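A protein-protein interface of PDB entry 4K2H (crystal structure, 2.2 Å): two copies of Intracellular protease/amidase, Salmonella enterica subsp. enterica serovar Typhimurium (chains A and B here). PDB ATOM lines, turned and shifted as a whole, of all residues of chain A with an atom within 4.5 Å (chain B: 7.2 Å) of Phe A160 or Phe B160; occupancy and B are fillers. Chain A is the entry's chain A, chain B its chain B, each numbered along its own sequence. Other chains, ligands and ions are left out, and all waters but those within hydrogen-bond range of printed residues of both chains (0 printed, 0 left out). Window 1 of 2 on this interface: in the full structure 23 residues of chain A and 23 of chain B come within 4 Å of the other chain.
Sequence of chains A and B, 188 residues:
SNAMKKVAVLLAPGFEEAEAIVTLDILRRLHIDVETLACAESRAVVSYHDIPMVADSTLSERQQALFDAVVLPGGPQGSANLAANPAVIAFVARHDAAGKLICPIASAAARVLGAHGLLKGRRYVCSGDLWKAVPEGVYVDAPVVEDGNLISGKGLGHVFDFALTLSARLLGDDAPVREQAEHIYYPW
O of Ile A184 sits at hydrogen-bond distance from N of Gly B157, at 2.8 Å.
Val A22 touches its own counterpart, Val B22. Leu A156 touches Phe B160, and with the chains exchanged Phe A160 touches Leu B156. Leu A156 touches Ile B184, and with the chains exchanged Ile A184 touches Leu B156. Phe B160 touches its own counterpart, Phe A160. 12 positions are printed for both chains. Of the 8 pairs that touch across the chains among the printed residues, 6 have their exchanged pair printed and touching as well.
Among the printed residues, merely in contact across the chains: Leu A156 with Asp B25 (3.1 Å), Val A22 with Val B22 (3.5 Å), Leu A156 with Phe B160 (3.6 Å), Phe A160 with Leu B156 (3.6 Å), Phe A160 with Phe B160 (3.9 Å), Leu A156 with Ile B184 (3.9 Å) and Ile A184 with Leu B156 (3.98 Å).
Printed residues of chain B within 4 Å of Val A22: Val B22 (3.5 Å). Of the printed residues of chain A, Asp B25 touches Leu A156. Trp B188 touches none of the printed residues of chain A.
Along chain B the printed residues that touch a printed residue of chain A span positions 22 to 184. Of the 12 printed residues of chain A, 4 touch a printed residue of chain B. Among the printed residues, no Asp or Glu carboxylate lies within 4 Å of a Lys or Arg side-chain nitrogen of the other chain.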
ATOM      1  N   VAL A  22      21.567  33.396   9.631  1.00  0.00           N
ATOM      2  CA  VAL A  22      20.399  32.986  10.434  1.00  0.00           C
ATOM      3  C   VAL A  22      19.814  34.237  11.096  1.00  0.00           C
ATOM      4  O   VAL A  22      18.601  34.435  11.061  1.00  0.00           O
ATOM      5  CB  VAL A  22      20.699  31.865  11.447  1.00  0.00           C
ATOM      6  CG1 VAL A  22      19.482  31.549  12.323  1.00  0.00           C
ATOM      7  CG2 VAL A  22      21.097  30.587  10.740  1.00  0.00           C
ATOM      8  N   ILE A  26      16.001  35.602  10.448  1.00  0.00           N
ATOM      9  CA  ILE A  26      14.988  35.743  11.521  1.00  0.00           C
ATOM     10  C   ILE A  26      14.434  37.171  11.525  1.00  0.00           C
ATOM     11  O   ILE A  26      13.213  37.379  11.460  1.00  0.00           O
ATOM     12  CB  ILE A  26      15.583  35.400  12.897  1.00  0.00           C
ATOM     13  CG1 ILE A  26      15.982  33.921  12.945  1.00  0.00           C
ATOM     14  CG2 ILE A  26      14.612  35.733  14.031  1.00  0.00           C
ATOM     15  CD1 ILE A  26      14.838  32.963  12.726  1.00  0.00           C
ATOM     16  N   LEU A 156      27.391  29.552  17.209  1.00  0.00           N
ATOM     17  CA  LEU A 156      26.461  29.167  16.154  1.00  0.00           C
ATOM     18  C   LEU A 156      25.334  28.268  16.633  1.00  0.00           C
ATOM     19  O   LEU A 156      24.187  28.439  16.219  1.00  0.00           O
ATOM     20  CB  LEU A 156      27.194  28.536  14.966  1.00  0.00           C
ATOM     21  CG  LEU A 156      26.333  28.037  13.792  1.00  0.00           C
ATOM     22  CD1 LEU A 156      25.502  29.158  13.214  1.00  0.00           C
ATOM     23  CD2 LEU A 156      27.193  27.343  12.721  1.00  0.00           C
ATOM     24  N   HIS A 158      23.746  28.472  19.180  1.00  0.00           N
ATOM     25  CA  HIS A 158      22.713  29.242  19.886  1.00  0.00           C
ATOM     26  C   HIS A 158      22.188  30.422  19.094  1.00  0.00           C
ATOM     27  O   HIS A 158      21.516  31.276  19.655  1.00  0.00           O
ATOM     28  CB  HIS A 158      23.255  29.745  21.208  1.00  0.00           C
ATOM     29  CG  HIS A 158      23.702  28.663  22.124  1.00  0.00           C
ATOM     30  ND1 HIS A 158      22.820  27.811  22.740  1.00  0.00           N
ATOM     31  CD2 HIS A 158      24.934  28.323  22.569  1.00  0.00           C
ATOM     32  CE1 HIS A 158      23.487  26.969  23.508  1.00  0.00           C
ATOM     33  NE2 HIS A 158      24.772  27.267  23.432  1.00  0.00           N
ATOM     34  N   VAL A 159      22.410  30.421  17.779  1.00  0.00           N
ATOM     35  CA  VAL A 159      22.096  31.575  16.952  1.00  0.00           C
ATOM     36  C   VAL A 159      20.603  31.888  16.884  1.00  0.00           C
ATOM     37  O   VAL A 159      20.222  33.043  16.827  1.00  0.00           O
ATOM     38  CB  VAL A 159      22.689  31.418  15.534  1.00  0.00           C
ATOM     39  CG1 VAL A 159      21.949  30.347  14.734  1.00  0.00           C
ATOM     40  CG2 VAL A 159      22.660  32.745  14.804  1.00  0.00           C
ATOM     41  N   PHE A 160      19.747  30.868  16.907  1.00  0.00           N
ATOM     42  CA  PHE A 160      18.303  31.114  16.897  1.00  0.00           C
ATOM     43  C   PHE A 160      17.898  31.865  18.153  1.00  0.00           C
ATOM     44  O   PHE A 160      17.175  32.867  18.082  1.00  0.00           O
ATOM     45  CB  PHE A 160      17.518  29.810  16.725  1.00  0.00           C
ATOM     46  CG  PHE A 160      17.568  29.246  15.313  1.00  0.00           C
ATOM     47  CD1 PHE A 160      16.926  29.901  14.265  1.00  0.00           C
ATOM     48  CD2 PHE A 160      18.241  28.048  15.040  1.00  0.00           C
ATOM     49  CE1 PHE A 160      16.970  29.394  12.974  1.00  0.00           C
ATOM     50  CE2 PHE A 160      18.283  27.534  13.750  1.00  0.00           C
ATOM     51  CZ  PHE A 160      17.650  28.209  12.710  1.00  0.00           C
ATOM     52  N   ASP A 161      18.399  31.409  19.297  1.00  0.00           N
ATOM     53  CA  ASP A 161      18.072  32.059  20.557  1.00  0.00           C
ATOM     54  C   ASP A 161      18.532  33.518  20.526  1.00  0.00           C
ATOM     55  O   ASP A 161      17.778  34.425  20.927  1.00  0.00           O
ATOM     56  CB  ASP A 161      18.692  31.311  21.742  1.00  0.00           C
ATOM     57  CG  ASP A 161      18.094  31.738  23.074  1.00  0.00           C
ATOM     58  OD1 ASP A 161      17.212  32.620  23.058  1.00  0.00           O
ATOM     59  OD2 ASP A 161      18.505  31.196  24.129  1.00  0.00           O
ATOM     60  N   PHE A 162      19.746  33.740  20.032  1.00  0.00           N
ATOM     61  CA  PHE A 162      20.323  35.081  19.895  1.00  0.00           C
ATOM     62  C   PHE A 162      19.460  35.974  19.019  1.00  0.00           C
ATOM     63  O   PHE A 162      19.131  37.109  19.403  1.00  0.00           O
ATOM     64  CB  PHE A 162      21.756  34.957  19.356  1.00  0.00           C
ATOM     65  CG  PHE A 162      22.362  36.255  18.869  1.00  0.00           C
ATOM     66  CD1 PHE A 162      22.996  37.128  19.756  1.00  0.00           C
ATOM     67  CD2 PHE A 162      22.334  36.581  17.516  1.00  0.00           C
ATOM     68  CE1 PHE A 162      23.571  38.311  19.301  1.00  0.00           C
ATOM     69  CE2 PHE A 162      22.918  37.751  17.058  1.00  0.00           C
ATOM     70  CZ  PHE A 162      23.519  38.628  17.963  1.00  0.00           C
ATOM     71  N   ALA A 163      19.101  35.458  17.846  1.00  0.00           N
ATOM     72  CA  ALA A 163      18.293  36.200  16.885  1.00  0.00           C
ATOM     73  C   ALA A 163      16.875  36.492  17.405  1.00  0.00           C
ATOM     74  O   ALA A 163      16.367  37.605  17.262  1.00  0.00           O
ATOM     75  CB  ALA A 163      18.223  35.443  15.560  1.00  0.00           C
ATOM     76  N   LEU A 164      16.231  35.485  18.004  1.00  0.00           N
ATOM     77  CA  LEU A 164      14.870  35.690  18.526  1.00  0.00           C
ATOM     78  C   LEU A 164      14.901  36.693  19.682  1.00  0.00           C
ATOM     79  O   LEU A 164      14.097  37.604  19.724  1.00  0.00           O
ATOM     80  CB  LEU A 164      14.218  34.365  18.896  1.00  0.00           C
ATOM     81  CG  LEU A 164      14.051  33.431  17.688  1.00  0.00           C
ATOM     82  CD1 LEU A 164      13.787  32.016  18.153  1.00  0.00           C
ATOM     83  CD2 LEU A 164      12.972  33.857  16.691  1.00  0.00           C
ATOM     84  N   ILE A 184       8.749  28.198  12.149  1.00  0.00           N
ATOM     85  CA  ILE A 184       9.946  27.499  11.667  1.00  0.00           C
ATOM     86  C   ILE A 184      10.329  26.312  12.560  1.00  0.00           C
ATOM     87  O   ILE A 184      11.359  25.665  12.334  1.00  0.00           O
ATOM     88  CB  ILE A 184      11.160  28.456  11.478  1.00  0.00           C
ATOM     89  CG1 ILE A 184      11.537  29.164  12.779  1.00  0.00           C
ATOM     90  CG2 ILE A 184      10.846  29.486  10.400  1.00  0.00           C
ATOM     91  CD1 ILE A 184      12.972  29.627  12.848  1.00  0.00           C
ATOM     92  N   TYR A 186      11.123  26.108  15.820  1.00  0.00           N
ATOM     93  CA  TYR A 186      12.147  26.275  16.841  1.00  0.00           C
ATOM     94  C   TYR A 186      11.524  26.543  18.218  1.00  0.00           C
ATOM     95  O   TYR A 186      10.881  27.553  18.396  1.00  0.00           O
ATOM     96  CB  TYR A 186      13.091  27.425  16.498  1.00  0.00           C
ATOM     97  CG  TYR A 186      14.240  27.491  17.462  1.00  0.00           C
ATOM     98  CD1 TYR A 186      15.305  26.594  17.366  1.00  0.00           C
ATOM     99  CD2 TYR A 186      14.251  28.404  18.496  1.00  0.00           C
ATOM    100  CE1 TYR A 186      16.359  26.634  18.275  1.00  0.00           C
ATOM    101  CE2 TYR A 186      15.303  28.456  19.390  1.00  0.00           C
ATOM    102  CZ  TYR A 186      16.342  27.565  19.281  1.00  0.00           C
ATOM    103  OH  TYR A 186      17.380  27.618  20.173  1.00  0.00           O
ATOM    104  N   ALA B  18      19.004  30.535   4.711  1.00  0.00           N
ATOM    105  CA  ALA B  18      19.362  30.028   6.052  1.00  0.00           C
ATOM    106  C   ALA B  18      19.539  28.518   6.086  1.00  0.00           C
ATOM    107  O   ALA B  18      20.446  27.996   6.691  1.00  0.00           O
ATOM    108  CB  ALA B  18      18.337  30.481   7.074  1.00  0.00           C
ATOM    109  N   VAL B  22      23.420  27.068   6.608  1.00  0.00           N
ATOM    110  CA  VAL B  22      23.769  26.339   7.802  1.00  0.00           C
ATOM    111  C   VAL B  22      24.232  24.954   7.404  1.00  0.00           C
ATOM    112  O   VAL B  22      25.203  24.460   7.931  1.00  0.00           O
ATOM    113  CB  VAL B  22      22.598  26.232   8.783  1.00  0.00           C
ATOM    114  CG1 VAL B  22      23.018  25.407   9.987  1.00  0.00           C
ATOM    115  CG2 VAL B  22      22.137  27.629   9.233  1.00  0.00           C
ATOM    116  N   THR B  23      23.535  24.322   6.465  1.00  0.00           N
ATOM    117  CA  THR B  23      23.864  22.943   6.063  1.00  0.00           C
ATOM    118  C   THR B  23      25.260  22.981   5.500  1.00  0.00           C
ATOM    119  O   THR B  23      26.130  22.185   5.840  1.00  0.00           O
ATOM    120  CB  THR B  23      22.878  22.473   4.975  1.00  0.00           C
ATOM    121  OG1 THR B  23      21.572  22.429   5.534  1.00  0.00           O
ATOM    122  CG2 THR B  23      23.209  21.115   4.416  1.00  0.00           C
ATOM    123  N   ASP B  25      27.593  25.333   5.997  1.00  0.00           N
ATOM    124  CA  ASP B  25      28.554  25.628   7.071  1.00  0.00           C
ATOM    125  C   ASP B  25      28.984  24.364   7.803  1.00  0.00           C
ATOM    126  O   ASP B  25      30.164  24.177   8.079  1.00  0.00           O
ATOM    127  CB  ASP B  25      27.938  26.656   8.050  1.00  0.00           C
ATOM    128  CG  ASP B  25      28.664  26.733   9.385  1.00  0.00           C
ATOM    129  OD1 ASP B  25      28.448  25.850  10.254  1.00  0.00           O
ATOM    130  OD2 ASP B  25      29.443  27.680   9.584  1.00  0.00           O
ATOM    131  N   ILE B  26      28.006  23.511   8.124  1.00  0.00           N
ATOM    132  CA  ILE B  26      28.250  22.278   8.872  1.00  0.00           C
ATOM    133  C   ILE B  26      29.103  21.280   8.061  1.00  0.00           C
ATOM    134  O   ILE B  26      30.097  20.722   8.557  1.00  0.00           O
ATOM    135  CB  ILE B  26      26.923  21.576   9.292  1.00  0.00           C
ATOM    136  CG1 ILE B  26      26.130  22.473  10.262  1.00  0.00           C
ATOM    137  CG2 ILE B  26      27.205  20.226   9.930  1.00  0.00           C
ATOM    138  CD1 ILE B  26      26.887  22.810  11.534  1.00  0.00           C
ATOM    139  N   ILE B 105      14.916  19.921   2.060  1.00  0.00           N
ATOM    140  CA  ILE B 105      14.569  20.499   3.350  1.00  0.00           C
ATOM    141  C   ILE B 105      13.409  21.459   3.175  1.00  0.00           C
ATOM    142  O   ILE B 105      13.260  22.091   2.121  1.00  0.00           O
ATOM    143  CB  ILE B 105      15.794  21.062   4.136  1.00  0.00           C
ATOM    144  CG1 ILE B 105      15.340  21.626   5.482  1.00  0.00           C
ATOM    145  CG2 ILE B 105      16.546  22.120   3.371  1.00  0.00           C
ATOM    146  CD1 ILE B 105      16.418  21.737   6.558  1.00  0.00           C
ATOM    147  N   VAL B 144      13.672  15.108  11.179  1.00  0.00           N
ATOM    148  CA  VAL B 144      14.410  14.539  10.060  1.00  0.00           C
ATOM    149  C   VAL B 144      13.840  13.172   9.774  1.00  0.00           C
ATOM    150  O   VAL B 144      13.513  12.427  10.681  1.00  0.00           O
ATOM    151  CB  VAL B 144      15.881  14.372  10.414  1.00  0.00           C
ATOM    152  CG1 VAL B 144      16.664  13.793   9.248  1.00  0.00           C
ATOM    153  CG2 VAL B 144      16.481  15.717  10.827  1.00  0.00           C
ATOM    154  N   GLY B 155      12.112  21.694   8.539  1.00  0.00           N
ATOM    155  CA  GLY B 155      12.136  23.149   8.357  1.00  0.00           C
ATOM    156  C   GLY B 155      13.366  23.767   8.983  1.00  0.00           C
ATOM    157  O   GLY B 155      14.170  23.087   9.596  1.00  0.00           O
ATOM    158  N   LEU B 156      13.506  25.072   8.835  1.00  0.00           N
ATOM    159  CA  LEU B 156      14.702  25.765   9.291  1.00  0.00           C
ATOM    160  C   LEU B 156      15.017  25.517  10.773  1.00  0.00           C
ATOM    161  O   LEU B 156      16.181  25.330  11.141  1.00  0.00           O
ATOM    162  CB  LEU B 156      14.573  27.254   9.014  1.00  0.00           C
ATOM    163  CG  LEU B 156      15.767  28.077   9.490  1.00  0.00           C
ATOM    164  CD1 LEU B 156      17.017  27.745   8.664  1.00  0.00           C
ATOM    165  CD2 LEU B 156      15.412  29.540   9.408  1.00  0.00           C
ATOM    166  N   GLY B 157      14.010  25.476  11.626  1.00  0.00           N
ATOM    167  CA  GLY B 157      14.263  25.246  13.072  1.00  0.00           C
ATOM    168  C   GLY B 157      15.023  23.958  13.342  1.00  0.00           C
ATOM    169  O   GLY B 157      15.695  23.839  14.338  1.00  0.00           O
ATOM    170  N   HIS B 158      14.903  22.988  12.440  1.00  0.00           N
ATOM    171  CA  HIS B 158      15.592  21.690  12.559  1.00  0.00           C
ATOM    172  C   HIS B 158      16.815  21.498  11.636  1.00  0.00           C
ATOM    173  O   HIS B 158      17.238  20.350  11.382  1.00  0.00           O
ATOM    174  CB  HIS B 158      14.579  20.571  12.253  1.00  0.00           C
ATOM    175  CG  HIS B 158      13.443  20.516  13.209  1.00  0.00           C
ATOM    176  ND1 HIS B 158      13.619  20.239  14.541  1.00  0.00           N
ATOM    177  CD2 HIS B 158      12.113  20.657  13.024  1.00  0.00           C
ATOM    178  CE1 HIS B 158      12.448  20.229  15.144  1.00  0.00           C
ATOM    179  NE2 HIS B 158      11.518  20.483  14.245  1.00  0.00           N
ATOM    180  N   VAL B 159      17.418  22.592  11.171  1.00  0.00           N
ATOM    181  CA  VAL B 159      18.482  22.511  10.150  1.00  0.00           C
ATOM    182  C   VAL B 159      19.769  21.861  10.685  1.00  0.00           C
ATOM    183  O   VAL B 159      20.455  21.091   9.972  1.00  0.00           O
ATOM    184  CB  VAL B 159      18.766  23.902   9.536  1.00  0.00           C
ATOM    185  CG1 VAL B 159      19.409  24.864  10.539  1.00  0.00           C
ATOM    186  CG2 VAL B 159      19.614  23.787   8.281  1.00  0.00           C
ATOM    187  N   PHE B 160      20.074  22.118  11.955  1.00  0.00           N
ATOM    188  CA  PHE B 160      21.214  21.471  12.559  1.00  0.00           C
ATOM    189  C   PHE B 160      21.023  19.949  12.594  1.00  0.00           C
ATOM    190  O   PHE B 160      21.932  19.207  12.200  1.00  0.00           O
ATOM    191  CB  PHE B 160      21.530  22.040  13.948  1.00  0.00           C
ATOM    192  CG  PHE B 160      22.007  23.456  13.927  1.00  0.00           C
ATOM    193  CD1 PHE B 160      23.274  23.760  13.446  1.00  0.00           C
ATOM    194  CD2 PHE B 160      21.204  24.493  14.390  1.00  0.00           C
ATOM    195  CE1 PHE B 160      23.737  25.059  13.417  1.00  0.00           C
ATOM    196  CE2 PHE B 160      21.670  25.801  14.373  1.00  0.00           C
ATOM    197  CZ  PHE B 160      22.931  26.088  13.874  1.00  0.00           C
ATOM    198  N   ASP B 161      19.849  19.479  13.009  1.00  0.00           N
ATOM    199  CA  ASP B 161      19.589  18.041  13.028  1.00  0.00           C
ATOM    200  C   ASP B 161      19.778  17.519  11.606  1.00  0.00           C
ATOM    201  O   ASP B 161      20.480  16.550  11.382  1.00  0.00           O
ATOM    202  CB  ASP B 161      18.184  17.706  13.592  1.00  0.00           C
ATOM    203  CG  ASP B 161      18.027  16.216  14.006  1.00  0.00           C
ATOM    204  OD1 ASP B 161      18.842  15.383  13.522  1.00  0.00           O
ATOM    205  OD2 ASP B 161      17.086  15.854  14.804  1.00  0.00           O
ATOM    206  N   PHE B 162      19.151  18.181  10.652  1.00  0.00           N
ATOM    207  CA  PHE B 162      19.239  17.777   9.269  1.00  0.00           C
ATOM    208  C   PHE B 162      20.686  17.684   8.817  1.00  0.00           C
ATOM    209  O   PHE B 162      21.109  16.665   8.331  1.00  0.00           O
ATOM    210  CB  PHE B 162      18.475  18.757   8.415  1.00  0.00           C
ATOM    211  CG  PHE B 162      18.694  18.600   6.938  1.00  0.00           C
ATOM    212  CD1 PHE B 162      18.027  17.620   6.227  1.00  0.00           C
ATOM    213  CD2 PHE B 162      19.515  19.490   6.247  1.00  0.00           C
ATOM    214  CE1 PHE B 162      18.177  17.521   4.869  1.00  0.00           C
ATOM    215  CE2 PHE B 162      19.686  19.378   4.884  1.00  0.00           C
ATOM    216  CZ  PHE B 162      19.011  18.398   4.187  1.00  0.00           C
ATOM    217  N   ALA B 163      21.448  18.740   9.048  1.00  0.00           N
ATOM    218  CA  ALA B 163      22.827  18.813   8.581  1.00  0.00           C
ATOM    219  C   ALA B 163      23.733  17.855   9.307  1.00  0.00           C
ATOM    220  O   ALA B 163      24.620  17.228   8.696  1.00  0.00           O
ATOM    221  CB  ALA B 163      23.350  20.237   8.692  1.00  0.00           C
ATOM    222  N   LEU B 164      23.499  17.687  10.613  1.00  0.00           N
ATOM    223  CA  LEU B 164      24.280  16.716  11.367  1.00  0.00           C
ATOM    224  C   LEU B 164      23.956  15.283  10.956  1.00  0.00           C
ATOM    225  O   LEU B 164      24.864  14.448  10.845  1.00  0.00           O
ATOM    226  CB  LEU B 164      24.189  16.958  12.865  1.00  0.00           C
ATOM    227  CG  LEU B 164      24.837  18.311  13.265  1.00  0.00           C
ATOM    228  CD1 LEU B 164      24.430  18.722  14.664  1.00  0.00           C
ATOM    229  CD2 LEU B 164      26.347  18.270  13.206  1.00  0.00           C
ATOM    230  N   THR B 165      22.692  15.003  10.665  1.00  0.00           N
ATOM    231  CA  THR B 165      22.338  13.686  10.153  1.00  0.00           C
ATOM    232  C   THR B 165      22.960  13.435   8.792  1.00  0.00           C
ATOM    233  O   THR B 165      23.605  12.420   8.563  1.00  0.00           O
ATOM    234  CB  THR B 165      20.814  13.504  10.098  1.00  0.00           C
ATOM    235  OG1 THR B 165      20.283  13.727  11.408  1.00  0.00           O
ATOM    236  CG2 THR B 165      20.423  12.070   9.631  1.00  0.00           C
ATOM    237  N   LEU B 166      22.807  14.361   7.869  1.00  0.00           N
ATOM    238  CA  LEU B 166      23.493  14.193   6.609  1.00  0.00           C
ATOM    239  C   LEU B 166      24.979  13.901   6.780  1.00  0.00           C
ATOM    240  O   LEU B 166      25.526  12.938   6.195  1.00  0.00           O
ATOM    241  CB  LEU B 166      23.344  15.470   5.788  1.00  0.00           C
ATOM    242  CG  LEU B 166      23.924  15.431   4.402  1.00  0.00           C
ATOM    243  CD1 LEU B 166      23.491  14.150   3.685  1.00  0.00           C
ATOM    244  CD2 LEU B 166      23.444  16.681   3.715  1.00  0.00           C
ATOM    245  N   SER B 167      25.646  14.733   7.579  1.00  0.00           N
ATOM    246  CA  SER B 167      27.073  14.617   7.752  1.00  0.00           C
ATOM    247  C   SER B 167      27.511  13.273   8.294  1.00  0.00           C
ATOM    248  O   SER B 167      28.471  12.673   7.792  1.00  0.00           O
ATOM    249  CB  SER B 167      27.595  15.728   8.653  1.00  0.00           C
ATOM    250  OG  SER B 167      27.312  16.999   8.103  1.00  0.00           O
ATOM    251  N   ILE B 184      30.467  24.029  18.255  1.00  0.00           N
ATOM    252  CA  ILE B 184      29.520  25.146  18.088  1.00  0.00           C
ATOM    253  C   ILE B 184      28.406  25.207  19.137  1.00  0.00           C
ATOM    254  O   ILE B 184      27.478  25.992  19.024  1.00  0.00           O
ATOM    255  CB  ILE B 184      28.911  25.141  16.693  1.00  0.00           C
ATOM    256  CG1 ILE B 184      28.193  23.836  16.438  1.00  0.00           C
ATOM    257  CG2 ILE B 184      30.015  25.352  15.650  1.00  0.00           C
ATOM    258  CD1 ILE B 184      27.158  23.935  15.349  1.00  0.00           C
ATOM    259  N   TYR B 186      26.146  22.897  20.026  1.00  0.00           N
ATOM    260  CA  TYR B 186      24.900  22.245  19.632  1.00  0.00           C
ATOM    261  C   TYR B 186      24.930  20.809  20.145  1.00  0.00           C
ATOM    262  O   TYR B 186      25.857  20.053  19.834  1.00  0.00           O
ATOM    263  CB  TYR B 186      24.709  22.240  18.112  1.00  0.00           C
ATOM    264  CG  TYR B 186      23.336  21.739  17.752  1.00  0.00           C
ATOM    265  CD1 TYR B 186      22.268  22.616  17.698  1.00  0.00           C
ATOM    266  CD2 TYR B 186      23.086  20.386  17.583  1.00  0.00           C
ATOM    267  CE1 TYR B 186      20.995  22.175  17.425  1.00  0.00           C
ATOM    268  CE2 TYR B 186      21.813  19.934  17.318  1.00  0.00           C
ATOM    269  CZ  TYR B 186      20.774  20.836  17.238  1.00  0.00           C
ATOM    270  OH  TYR B 186      19.492  20.425  16.968  1.00  0.00           O
ATOM    271  N   TRP B 188      24.608  17.017  20.370  1.00  0.00           N
ATOM    272  CA  TRP B 188      24.485  15.893  19.422  1.00  0.00           C
ATOM    273  C   TRP B 188      25.383  14.756  19.855  1.00  0.00           C
ATOM    274  O   TRP B 188      26.517  15.013  20.268  1.00  0.00           O
ATOM    275  CB  TRP B 188      24.922  16.316  18.007  1.00  0.00           C
ATOM    276  CG  TRP B 188      24.534  15.360  16.948  1.00  0.00           C
ATOM    277  CD1 TRP B 188      23.330  15.318  16.282  1.00  0.00           C
ATOM    278  CD2 TRP B 188      25.341  14.331  16.377  1.00  0.00           C
ATOM    279  NE1 TRP B 188      23.340  14.294  15.353  1.00  0.00           N
ATOM    280  CE2 TRP B 188      24.557  13.673  15.394  1.00  0.00           C
ATOM    281  CE3 TRP B 188      26.641  13.891  16.595  1.00  0.00           C
ATOM    282  CZ2 TRP B 188      25.046  12.597  14.640  1.00  0.00           C
ATOM    283  CZ3 TRP B 188      27.127  12.818  15.843  1.00  0.00           C
ATOM    284  CH2 TRP B 188      26.327  12.173  14.894  1.00  0.00           C
ATOM    285  OXT TRP B 188      25.038  13.570  19.802  1.00  0.00           O
